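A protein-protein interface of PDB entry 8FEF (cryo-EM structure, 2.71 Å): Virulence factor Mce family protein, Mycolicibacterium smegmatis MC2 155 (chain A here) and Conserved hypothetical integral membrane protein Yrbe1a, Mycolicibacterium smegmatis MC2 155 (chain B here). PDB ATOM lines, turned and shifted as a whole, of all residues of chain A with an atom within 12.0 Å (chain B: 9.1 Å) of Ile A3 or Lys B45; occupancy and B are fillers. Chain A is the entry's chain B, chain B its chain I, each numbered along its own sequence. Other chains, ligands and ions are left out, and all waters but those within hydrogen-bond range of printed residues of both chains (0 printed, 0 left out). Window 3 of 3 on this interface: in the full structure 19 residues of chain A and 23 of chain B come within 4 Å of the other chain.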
ATOM      1  N   SER A   2      19.105  10.386  -9.144  1.00  0.00           N
ATOM      2  CA  SER A   2      18.193   9.792  -8.174  1.00  0.00           C
ATOM      3  C   SER A   2      18.702   8.435  -7.701  1.00  0.00           C
ATOM      4  O   SER A   2      18.062   7.774  -6.884  1.00  0.00           O
ATOM      5  CB  SER A   2      16.792   9.649  -8.773  1.00  0.00           C
ATOM      6  OG  SER A   2      15.898   9.055  -7.847  1.00  0.00           O
ATOM      7  N   ILE A   3      19.856   8.023  -8.230  1.00  0.00           N
ATOM      8  CA  ILE A   3      20.437   6.741  -7.841  1.00  0.00           C
ATOM      9  C   ILE A   3      20.883   6.766  -6.383  1.00  0.00           C
ATOM     10  O   ILE A   3      20.839   5.736  -5.700  1.00  0.00           O
ATOM     11  CB  ILE A   3      21.586   6.362  -8.798  1.00  0.00           C
ATOM     12  CG1 ILE A   3      22.105   4.954  -8.493  1.00  0.00           C
ATOM     13  CG2 ILE A   3      22.711   7.392  -8.751  1.00  0.00           C
ATOM     14  CD1 ILE A   3      23.008   4.388  -9.567  1.00  0.00           C
ATOM     15  N   LYS A   4      21.318   7.925  -5.882  1.00  0.00           N
ATOM     16  CA  LYS A   4      21.739   8.030  -4.487  1.00  0.00           C
ATOM     17  C   LYS A   4      20.577   7.760  -3.536  1.00  0.00           C
ATOM     18  O   LYS A   4      20.711   7.002  -2.568  1.00  0.00           O
ATOM     19  CB  LYS A   4      22.339   9.413  -4.228  1.00  0.00           C
ATOM     20  CG  LYS A   4      23.469   9.426  -3.214  1.00  0.00           C
ATOM     21  CD  LYS A   4      24.692   8.696  -3.744  1.00  0.00           C
ATOM     22  CE  LYS A   4      25.914   8.966  -2.880  1.00  0.00           C
ATOM     23  NZ  LYS A   4      25.697   8.562  -1.464  1.00  0.00           N
ATOM     24  N   GLY A   5      19.421   8.374  -3.801  1.00  0.00           N
ATOM     25  CA  GLY A   5      18.262   8.145  -2.954  1.00  0.00           C
ATOM     26  C   GLY A   5      17.749   6.720  -3.042  1.00  0.00           C
ATOM     27  O   GLY A   5      17.326   6.140  -2.037  1.00  0.00           O
ATOM     28  N   THR A   6      17.772   6.141  -4.244  1.00  0.00           N
ATOM     29  CA  THR A   6      17.379   4.744  -4.403  1.00  0.00           C
ATOM     30  C   THR A   6      18.313   3.827  -3.626  1.00  0.00           C
ATOM     31  O   THR A   6      17.861   2.877  -2.979  1.00  0.00           O
ATOM     32  CB  THR A   6      17.362   4.369  -5.885  1.00  0.00           C
ATOM     33  OG1 THR A   6      16.400   5.177  -6.572  1.00  0.00           O
ATOM     34  CG2 THR A   6      17.000   2.904  -6.066  1.00  0.00           C
ATOM     35  N   LEU A   7      19.619   4.105  -3.669  1.00  0.00           N
ATOM     36  CA  LEU A   7      20.576   3.320  -2.897  1.00  0.00           C
ATOM     37  C   LEU A   7      20.321   3.454  -1.403  1.00  0.00           C
ATOM     38  O   LEU A   7      20.390   2.468  -0.666  1.00  0.00           O
ATOM     39  CB  LEU A   7      22.004   3.749  -3.233  1.00  0.00           C
ATOM     40  CG  LEU A   7      22.911   2.672  -3.829  1.00  0.00           C
ATOM     41  CD1 LEU A   7      24.333   3.188  -3.965  1.00  0.00           C
ATOM     42  CD2 LEU A   7      22.874   1.409  -2.984  1.00  0.00           C
ATOM     43  N   PHE A   8      20.028   4.671  -0.941  1.00  0.00           N
ATOM     44  CA  PHE A   8      19.731   4.894   0.472  1.00  0.00           C
ATOM     45  C   PHE A   8      18.505   4.097   0.913  1.00  0.00           C
ATOM     46  O   PHE A   8      18.537   3.389   1.932  1.00  0.00           O
ATOM     47  CB  PHE A   8      19.538   6.394   0.706  1.00  0.00           C
ATOM     48  CG  PHE A   8      19.016   6.750   2.066  1.00  0.00           C
ATOM     49  CD1 PHE A   8      19.851   6.736   3.171  1.00  0.00           C
ATOM     50  CD2 PHE A   8      17.698   7.144   2.233  1.00  0.00           C
ATOM     51  CE1 PHE A   8      19.373   7.081   4.420  1.00  0.00           C
ATOM     52  CE2 PHE A   8      17.215   7.490   3.479  1.00  0.00           C
ATOM     53  CZ  PHE A   8      18.054   7.460   4.573  1.00  0.00           C
ATOM     54  N   LYS A   9      17.416   4.192   0.141  1.00  0.00           N
ATOM     55  CA  LYS A   9      16.190   3.473   0.480  1.00  0.00           C
ATOM     56  C   LYS A   9      16.406   1.964   0.450  1.00  0.00           C
ATOM     57  O   LYS A   9      15.959   1.247   1.355  1.00  0.00           O
ATOM     58  CB  LYS A   9      15.065   3.870  -0.476  1.00  0.00           C
ATOM     59  CG  LYS A   9      14.669   5.333  -0.399  1.00  0.00           C
ATOM     60  CD  LYS A   9      13.610   5.670  -1.434  1.00  0.00           C
ATOM     61  CE  LYS A   9      13.230   7.141  -1.378  1.00  0.00           C
ATOM     62  NZ  LYS A   9      12.194   7.486  -2.389  1.00  0.00           N
ATOM     63  N   LEU A  10      17.086   1.467  -0.586  1.00  0.00           N
ATOM     64  CA  LEU A  10      17.330   0.035  -0.704  1.00  0.00           C
ATOM     65  C   LEU A  10      18.211  -0.462   0.431  1.00  0.00           C
ATOM     66  O   LEU A  10      17.980  -1.546   0.971  1.00  0.00           O
ATOM     67  CB  LEU A  10      17.965  -0.283  -2.057  1.00  0.00           C
ATOM     68  CG  LEU A  10      18.307  -1.755  -2.286  1.00  0.00           C
ATOM     69  CD1 LEU A  10      17.051  -2.600  -2.272  1.00  0.00           C
ATOM     70  CD2 LEU A  10      19.075  -1.950  -3.580  1.00  0.00           C
ATOM     71  N   GLY A  11      19.222   0.322   0.811  1.00  0.00           N
ATOM     72  CA  GLY A  11      20.078  -0.069   1.917  1.00  0.00           C
ATOM     73  C   GLY A  11      19.329  -0.152   3.231  1.00  0.00           C
ATOM     74  O   GLY A  11      19.491  -1.111   3.988  1.00  0.00           O
ATOM     75  N   ILE A  12      18.495   0.851   3.522  1.00  0.00           N
ATOM     76  CA  ILE A  12      17.722   0.825   4.765  1.00  0.00           C
ATOM     77  C   ILE A  12      16.761  -0.363   4.779  1.00  0.00           C
ATOM     78  O   ILE A  12      16.671  -1.103   5.772  1.00  0.00           O
ATOM     79  CB  ILE A  12      16.981   2.159   4.968  1.00  0.00           C
ATOM     80  CG1 ILE A  12      17.937   3.211   5.531  1.00  0.00           C
ATOM     81  CG2 ILE A  12      15.771   1.977   5.881  1.00  0.00           C
ATOM     82  CD1 ILE A  12      17.242   4.417   6.118  1.00  0.00           C
ATOM     83  N   PHE B  42      29.460  -7.065 -13.295  1.00  0.00           N
ATOM     84  CA  PHE B  42      28.100  -6.945 -12.795  1.00  0.00           C
ATOM     85  C   PHE B  42      27.589  -5.517 -12.950  1.00  0.00           C
ATOM     86  O   PHE B  42      28.351  -4.549 -12.887  1.00  0.00           O
ATOM     87  CB  PHE B  42      28.040  -7.372 -11.328  1.00  0.00           C
ATOM     88  CG  PHE B  42      26.650  -7.627 -10.826  1.00  0.00           C
ATOM     89  CD1 PHE B  42      25.972  -8.779 -11.185  1.00  0.00           C
ATOM     90  CD2 PHE B  42      26.028  -6.726  -9.984  1.00  0.00           C
ATOM     91  CE1 PHE B  42      24.696  -9.020 -10.722  1.00  0.00           C
ATOM     92  CE2 PHE B  42      24.753  -6.963  -9.516  1.00  0.00           C
ATOM     93  CZ  PHE B  42      24.086  -8.111  -9.886  1.00  0.00           C
ATOM     94  N   GLN B  43      26.280  -5.397 -13.159  1.00  0.00           N
ATOM     95  CA  GLN B  43      25.608  -4.107 -13.308  1.00  0.00           C
ATOM     96  C   GLN B  43      24.998  -3.739 -11.958  1.00  0.00           C
ATOM     97  O   GLN B  43      23.861  -4.098 -11.653  1.00  0.00           O
ATOM     98  CB  GLN B  43      24.550  -4.174 -14.404  1.00  0.00           C
ATOM     99  CG  GLN B  43      25.102  -4.459 -15.788  1.00  0.00           C
ATOM    100  CD  GLN B  43      25.691  -3.228 -16.443  1.00  0.00           C
ATOM    101  OE1 GLN B  43      25.237  -2.110 -16.210  1.00  0.00           O
ATOM    102  NE2 GLN B  43      26.711  -3.429 -17.268  1.00  0.00           N
ATOM    103  N   TRP B  44      25.769  -3.017 -11.143  1.00  0.00           N
ATOM    104  CA  TRP B  44      25.298  -2.651  -9.811  1.00  0.00           C
ATOM    105  C   TRP B  44      24.127  -1.676  -9.871  1.00  0.00           C
ATOM    106  O   TRP B  44      23.182  -1.787  -9.082  1.00  0.00           O
ATOM    107  CB  TRP B  44      26.446  -2.060  -8.992  1.00  0.00           C
ATOM    108  CG  TRP B  44      27.474  -3.070  -8.595  1.00  0.00           C
ATOM    109  CD1 TRP B  44      28.734  -3.202  -9.102  1.00  0.00           C
ATOM    110  CD2 TRP B  44      27.328  -4.102  -7.611  1.00  0.00           C
ATOM    111  NE1 TRP B  44      29.383  -4.248  -8.493  1.00  0.00           N
ATOM    112  CE2 TRP B  44      28.540  -4.818  -7.575  1.00  0.00           C
ATOM    113  CE3 TRP B  44      26.290  -4.488  -6.759  1.00  0.00           C
ATOM    114  CZ2 TRP B  44      28.743  -5.897  -6.718  1.00  0.00           C
ATOM    115  CZ3 TRP B  44      26.493  -5.559  -5.910  1.00  0.00           C
ATOM    116  CH2 TRP B  44      27.710  -6.252  -5.896  1.00  0.00           C
ATOM    117  N   LYS B  45      24.173  -0.714 -10.795  1.00  0.00           N
ATOM    118  CA  LYS B  45      23.128   0.303 -10.869  1.00  0.00           C
ATOM    119  C   LYS B  45      21.784  -0.312 -11.237  1.00  0.00           C
ATOM    120  O   LYS B  45      20.762  -0.041 -10.592  1.00  0.00           O
ATOM    121  CB  LYS B  45      23.523   1.380 -11.879  1.00  0.00           C
ATOM    122  CG  LYS B  45      24.982   1.793 -11.796  1.00  0.00           C
ATOM    123  CD  LYS B  45      25.337   2.796 -12.878  1.00  0.00           C
ATOM    124  CE  LYS B  45      26.818   3.131 -12.850  1.00  0.00           C
ATOM    125  NZ  LYS B  45      27.236   3.668 -11.527  1.00  0.00           N
ATOM    126  N   GLU B  46      21.767  -1.145 -12.280  1.00  0.00           N
ATOM    127  CA  GLU B  46      20.526  -1.786 -12.696  1.00  0.00           C
ATOM    128  C   GLU B  46      20.019  -2.741 -11.625  1.00  0.00           C
ATOM    129  O   GLU B  46      18.808  -2.857 -11.414  1.00  0.00           O
ATOM    130  CB  GLU B  46      20.729  -2.514 -14.024  1.00  0.00           C
ATOM    131  CG  GLU B  46      19.437  -2.836 -14.762  1.00  0.00           C
ATOM    132  CD  GLU B  46      18.791  -1.615 -15.389  1.00  0.00           C
ATOM    133  OE1 GLU B  46      19.449  -0.557 -15.466  1.00  0.00           O
ATOM    134  OE2 GLU B  46      17.618  -1.714 -15.805  1.00  0.00           O
ATOM    135  N   PHE B  47      20.934  -3.435 -10.941  1.00  0.00           N
ATOM    136  CA  PHE B  47      20.535  -4.318  -9.850  1.00  0.00           C
ATOM    137  C   PHE B  47      19.857  -3.540  -8.730  1.00  0.00           C
ATOM    138  O   PHE B  47      18.822  -3.970  -8.210  1.00  0.00           O
ATOM    139  CB  PHE B  47      21.752  -5.079  -9.322  1.00  0.00           C
ATOM    140  CG  PHE B  47      21.576  -5.621  -7.934  1.00  0.00           C
ATOM    141  CD1 PHE B  47      20.775  -6.723  -7.700  1.00  0.00           C
ATOM    142  CD2 PHE B  47      22.227  -5.036  -6.861  1.00  0.00           C
ATOM    143  CE1 PHE B  47      20.614  -7.220  -6.423  1.00  0.00           C
ATOM    144  CE2 PHE B  47      22.071  -5.531  -5.583  1.00  0.00           C
ATOM    145  CZ  PHE B  47      21.264  -6.625  -5.365  1.00  0.00           C
ATOM    146  N   VAL B  48      20.420  -2.391  -8.350  1.00  0.00           N
ATOM    147  CA  VAL B  48      19.813  -1.572  -7.304  1.00  0.00           C
ATOM    148  C   VAL B  48      18.441  -1.076  -7.743  1.00  0.00           C
ATOM    149  O   VAL B  48      17.469  -1.118  -6.973  1.00  0.00           O
ATOM    150  CB  VAL B  48      20.747  -0.405  -6.932  1.00  0.00           C
ATOM    151  CG1 VAL B  48      20.019   0.617  -6.075  1.00  0.00           C
ATOM    152  CG2 VAL B  48      21.972  -0.925  -6.205  1.00  0.00           C
ATOM    153  N   LEU B  49      18.340  -0.600  -8.989  1.00  0.00           N
ATOM    154  CA  LEU B  49      17.068  -0.078  -9.483  1.00  0.00           C
ATOM    155  C   LEU B  49      15.993  -1.159  -9.495  1.00  0.00           C
ATOM    156  O   LEU B  49      14.864  -0.931  -9.047  1.00  0.00           O
ATOM    157  CB  LEU B  49      17.252   0.518 -10.878  1.00  0.00           C
ATOM    158  CG  LEU B  49      18.080   1.800 -10.964  1.00  0.00           C
ATOM    159  CD1 LEU B  49      18.261   2.217 -12.411  1.00  0.00           C
ATOM    160  CD2 LEU B  49      17.423   2.911 -10.166  1.00  0.00           C
ATOM    161  N   GLN B  50      16.335  -2.354  -9.982  1.00  0.00           N
ATOM    162  CA  GLN B  50      15.357  -3.434 -10.036  1.00  0.00           C
ATOM    163  C   GLN B  50      15.008  -3.958  -8.650  1.00  0.00           C
ATOM    164  O   GLN B  50      13.856  -4.335  -8.410  1.00  0.00           O
ATOM    165  CB  GLN B  50      15.870  -4.564 -10.923  1.00  0.00           C
ATOM    166  CG  GLN B  50      16.036  -4.155 -12.368  1.00  0.00           C
ATOM    167  CD  GLN B  50      14.780  -3.536 -12.937  1.00  0.00           C
ATOM    168  OE1 GLN B  50      13.763  -4.209 -13.102  1.00  0.00           O
ATOM    169  NE2 GLN B  50      14.840  -2.245 -13.238  1.00  0.00           N
ATOM    170  N   SER B  51      15.976  -3.988  -7.728  1.00  0.00           N
ATOM    171  CA  SER B  51      15.680  -4.384  -6.357  1.00  0.00           C
ATOM    172  C   SER B  51      14.670  -3.436  -5.727  1.00  0.00           C
ATOM    173  O   SER B  51      13.678  -3.873  -5.133  1.00  0.00           O
ATOM    174  CB  SER B  51      16.965  -4.421  -5.530  1.00  0.00           C
ATOM    175  OG  SER B  51      17.902  -5.326  -6.080  1.00  0.00           O
ATOM    176  N   TRP B  52      14.900  -2.127  -5.862  1.00  0.00           N
ATOM    177  CA  TRP B  52      13.964  -1.172  -5.279  1.00  0.00           C
ATOM    178  C   TRP B  52      12.611  -1.230  -5.975  1.00  0.00           C
ATOM    179  O   TRP B  52      11.571  -1.067  -5.328  1.00  0.00           O
ATOM    180  CB  TRP B  52      14.533   0.244  -5.327  1.00  0.00           C
ATOM    181  CG  TRP B  52      13.571   1.264  -4.799  1.00  0.00           C
ATOM    182  CD1 TRP B  52      13.009   2.294  -5.493  1.00  0.00           C
ATOM    183  CD2 TRP B  52      13.035   1.337  -3.472  1.00  0.00           C
ATOM    184  NE1 TRP B  52      12.168   3.011  -4.679  1.00  0.00           N
ATOM    185  CE2 TRP B  52      12.164   2.443  -3.434  1.00  0.00           C
ATOM    186  CE3 TRP B  52      13.212   0.578  -2.310  1.00  0.00           C
ATOM    187  CZ2 TRP B  52      11.474   2.808  -2.282  1.00  0.00           C
ATOM    188  CZ3 TRP B  52      12.524   0.942  -1.170  1.00  0.00           C
ATOM    189  CH2 TRP B  52      11.666   2.046  -1.163  1.00  0.00           C
ATOM    190  N   PHE B  53      12.603  -1.463  -7.290  1.00  0.00           N
ATOM    191  CA  PHE B  53      11.344  -1.579  -8.019  1.00  0.00           C
ATOM    192  C   PHE B  53      10.523  -2.764  -7.522  1.00  0.00           C
ATOM    193  O   PHE B  53       9.326  -2.632  -7.242  1.00  0.00           O
ATOM    194  CB  PHE B  53      11.626  -1.699  -9.516  1.00  0.00           C
ATOM    195  CG  PHE B  53      10.412  -2.001 -10.341  1.00  0.00           C
ATOM    196  CD1 PHE B  53       9.371  -1.094 -10.425  1.00  0.00           C
ATOM    197  CD2 PHE B  53      10.319  -3.189 -11.045  1.00  0.00           C
ATOM    198  CE1 PHE B  53       8.255  -1.369 -11.188  1.00  0.00           C
ATOM    199  CE2 PHE B  53       9.207  -3.469 -11.810  1.00  0.00           C
ATOM    200  CZ  PHE B  53       8.174  -2.558 -11.881  1.00  0.00           C
ATOM    201  N   ARG B 145      23.130  -6.920 -19.622  1.00  0.00           N
ATOM    202  CA  ARG B 145      22.767  -5.597 -19.136  1.00  0.00           C
ATOM    203  C   ARG B 145      21.393  -5.562 -18.481  1.00  0.00           C
ATOM    204  O   ARG B 145      21.151  -4.705 -17.625  1.00  0.00           O
ATOM    205  CB  ARG B 145      22.826  -4.589 -20.291  1.00  0.00           C
ATOM    206  CG  ARG B 145      22.588  -3.141 -19.894  1.00  0.00           C
ATOM    207  CD  ARG B 145      23.053  -2.194 -20.981  1.00  0.00           C
ATOM    208  NE  ARG B 145      24.503  -2.209 -21.124  1.00  0.00           N
ATOM    209  CZ  ARG B 145      25.320  -1.321 -20.576  1.00  0.00           C
ATOM    210  NH1 ARG B 145      24.860  -0.317 -19.849  1.00  0.00           N
ATOM    211  NH2 ARG B 145      26.630  -1.441 -20.766  1.00  0.00           N
ATOM    212  N   PRO B 149      20.892  -8.365 -13.737  1.00  0.00           N
ATOM    213  CA  PRO B 149      20.443  -7.582 -12.574  1.00  0.00           C
ATOM    214  C   PRO B 149      19.024  -7.900 -12.143  1.00  0.00           C
ATOM    215  O   PRO B 149      18.741  -7.901 -10.942  1.00  0.00           O
ATOM    216  CB  PRO B 149      20.584  -6.130 -13.050  1.00  0.00           C
ATOM    217  CG  PRO B 149      20.610  -6.204 -14.513  1.00  0.00           C
ATOM    218  CD  PRO B 149      21.299  -7.473 -14.839  1.00  0.00           C
ATOM    219  N   ARG B 150      18.127  -8.198 -13.086  1.00  0.00           N
ATOM    220  CA  ARG B 150      16.746  -8.488 -12.719  1.00  0.00           C
ATOM    221  C   ARG B 150      16.626  -9.818 -11.982  1.00  0.00           C
ATOM    222  O   ARG B 150      15.886  -9.918 -11.000  1.00  0.00           O
ATOM    223  CB  ARG B 150      15.855  -8.468 -13.960  1.00  0.00           C
ATOM    224  CG  ARG B 150      15.618  -7.069 -14.489  1.00  0.00           C
ATOM    225  CD  ARG B 150      15.095  -7.063 -15.910  1.00  0.00           C
ATOM    226  NE  ARG B 150      15.595  -5.900 -16.635  1.00  0.00           N
ATOM    227  CZ  ARG B 150      15.049  -4.693 -16.582  1.00  0.00           C
ATOM    228  NH1 ARG B 150      13.957  -4.458 -15.874  1.00  0.00           N
ATOM    229  NH2 ARG B 150      15.615  -3.697 -17.254  1.00  0.00           N
ATOM    230  N   ALA B 153      18.167  -9.271  -8.492  1.00  0.00           N
ATOM    231  CA  ALA B 153      17.242  -8.485  -7.685  1.00  0.00           C
ATOM    232  C   ALA B 153      16.040  -9.313  -7.257  1.00  0.00           C
ATOM    233  O   ALA B 153      15.564  -9.185  -6.125  1.00  0.00           O
ATOM    234  CB  ALA B 153      16.789  -7.252  -8.464  1.00  0.00           C
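O of Ser A2 lies within hydrogen-bond range of OG1 of Thr A6 (3.1 Å). The side-chain hydroxyl (OG) of Ser B51 is in hydrogen-bond range of the backbone carbonyl oxygen (O) of Phe B47 (2.7 Å).
Among the printed residues, pairs that only touch across the chains: Lys A9 with Trp B52 (3.7 Å), Leu A10 with Val B48 (3.7 Å), Thr A6 with Trp B52 (3.7 Å), Leu A10 with Ser B51 (3.7 Å), Thr A6 with Val B48 (3.8 Å) and Ile A3 with Lys B45 (3.8 Å).
Hydrophobic or aromatic side chains of chain B within 4 Å of the printed part of chain A: Val B48 and Trp B52. Of the 11 printed residues of chain A, 4 touch a printed residue of chain B. Printed residues of chain A that touch a printed residue of chain B: Ile A3, Thr A6, Lys A9 and Leu A10. Hydrophobic or aromatic side chains of chain A that line the printed part of chain B: Ile A3 and Leu A10. Along chain A the printed residues that touch a printed residue of chain B span positions 3 to 10. Among the printed residues, 6 pairs touch across the chains. Among the printed residues, no Asp or Glu carboxylate lies within 4 Å of a Lys or Arg side-chain nitrogen of the other chain.
Printed residues of chain B within 4 Å of Ile A3: Lys B45 (3.8 Å). Of chain B, only Val B48 and Trp B52 come within 4 Å of Thr A6. Leu A7 touches none of the printed residues of chain B. Printed residues of chain B within 4 Å of Lys A9: Trp B52 (3.7 Å). Printed residues of chain B within 4 Å of Leu A10: Val B48 and Ser B51. Phe B42 touches none of the printed residues of chain A. Of chain A, only Thr A6 and Leu A10 come within 4 Å of Val B48. No residue of chain A comes within 4 Å of Leu B49. Of the printed residues of chain A, Ser B51 touches Leu A10 (3.7 Å). Of the printed residues of chain A, Trp B52 touches Thr A6 and Lys A9. The nearest residue of chain B that does not touch Ile A3 is Val B48 (5.2 Å). The nearest residue of chain A that does not touch Lys B45 is Thr A6 (6.6 Å). The nearest printed residue of chain B that does not touch Leu A10 is Trp B52 (4.2 Å).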
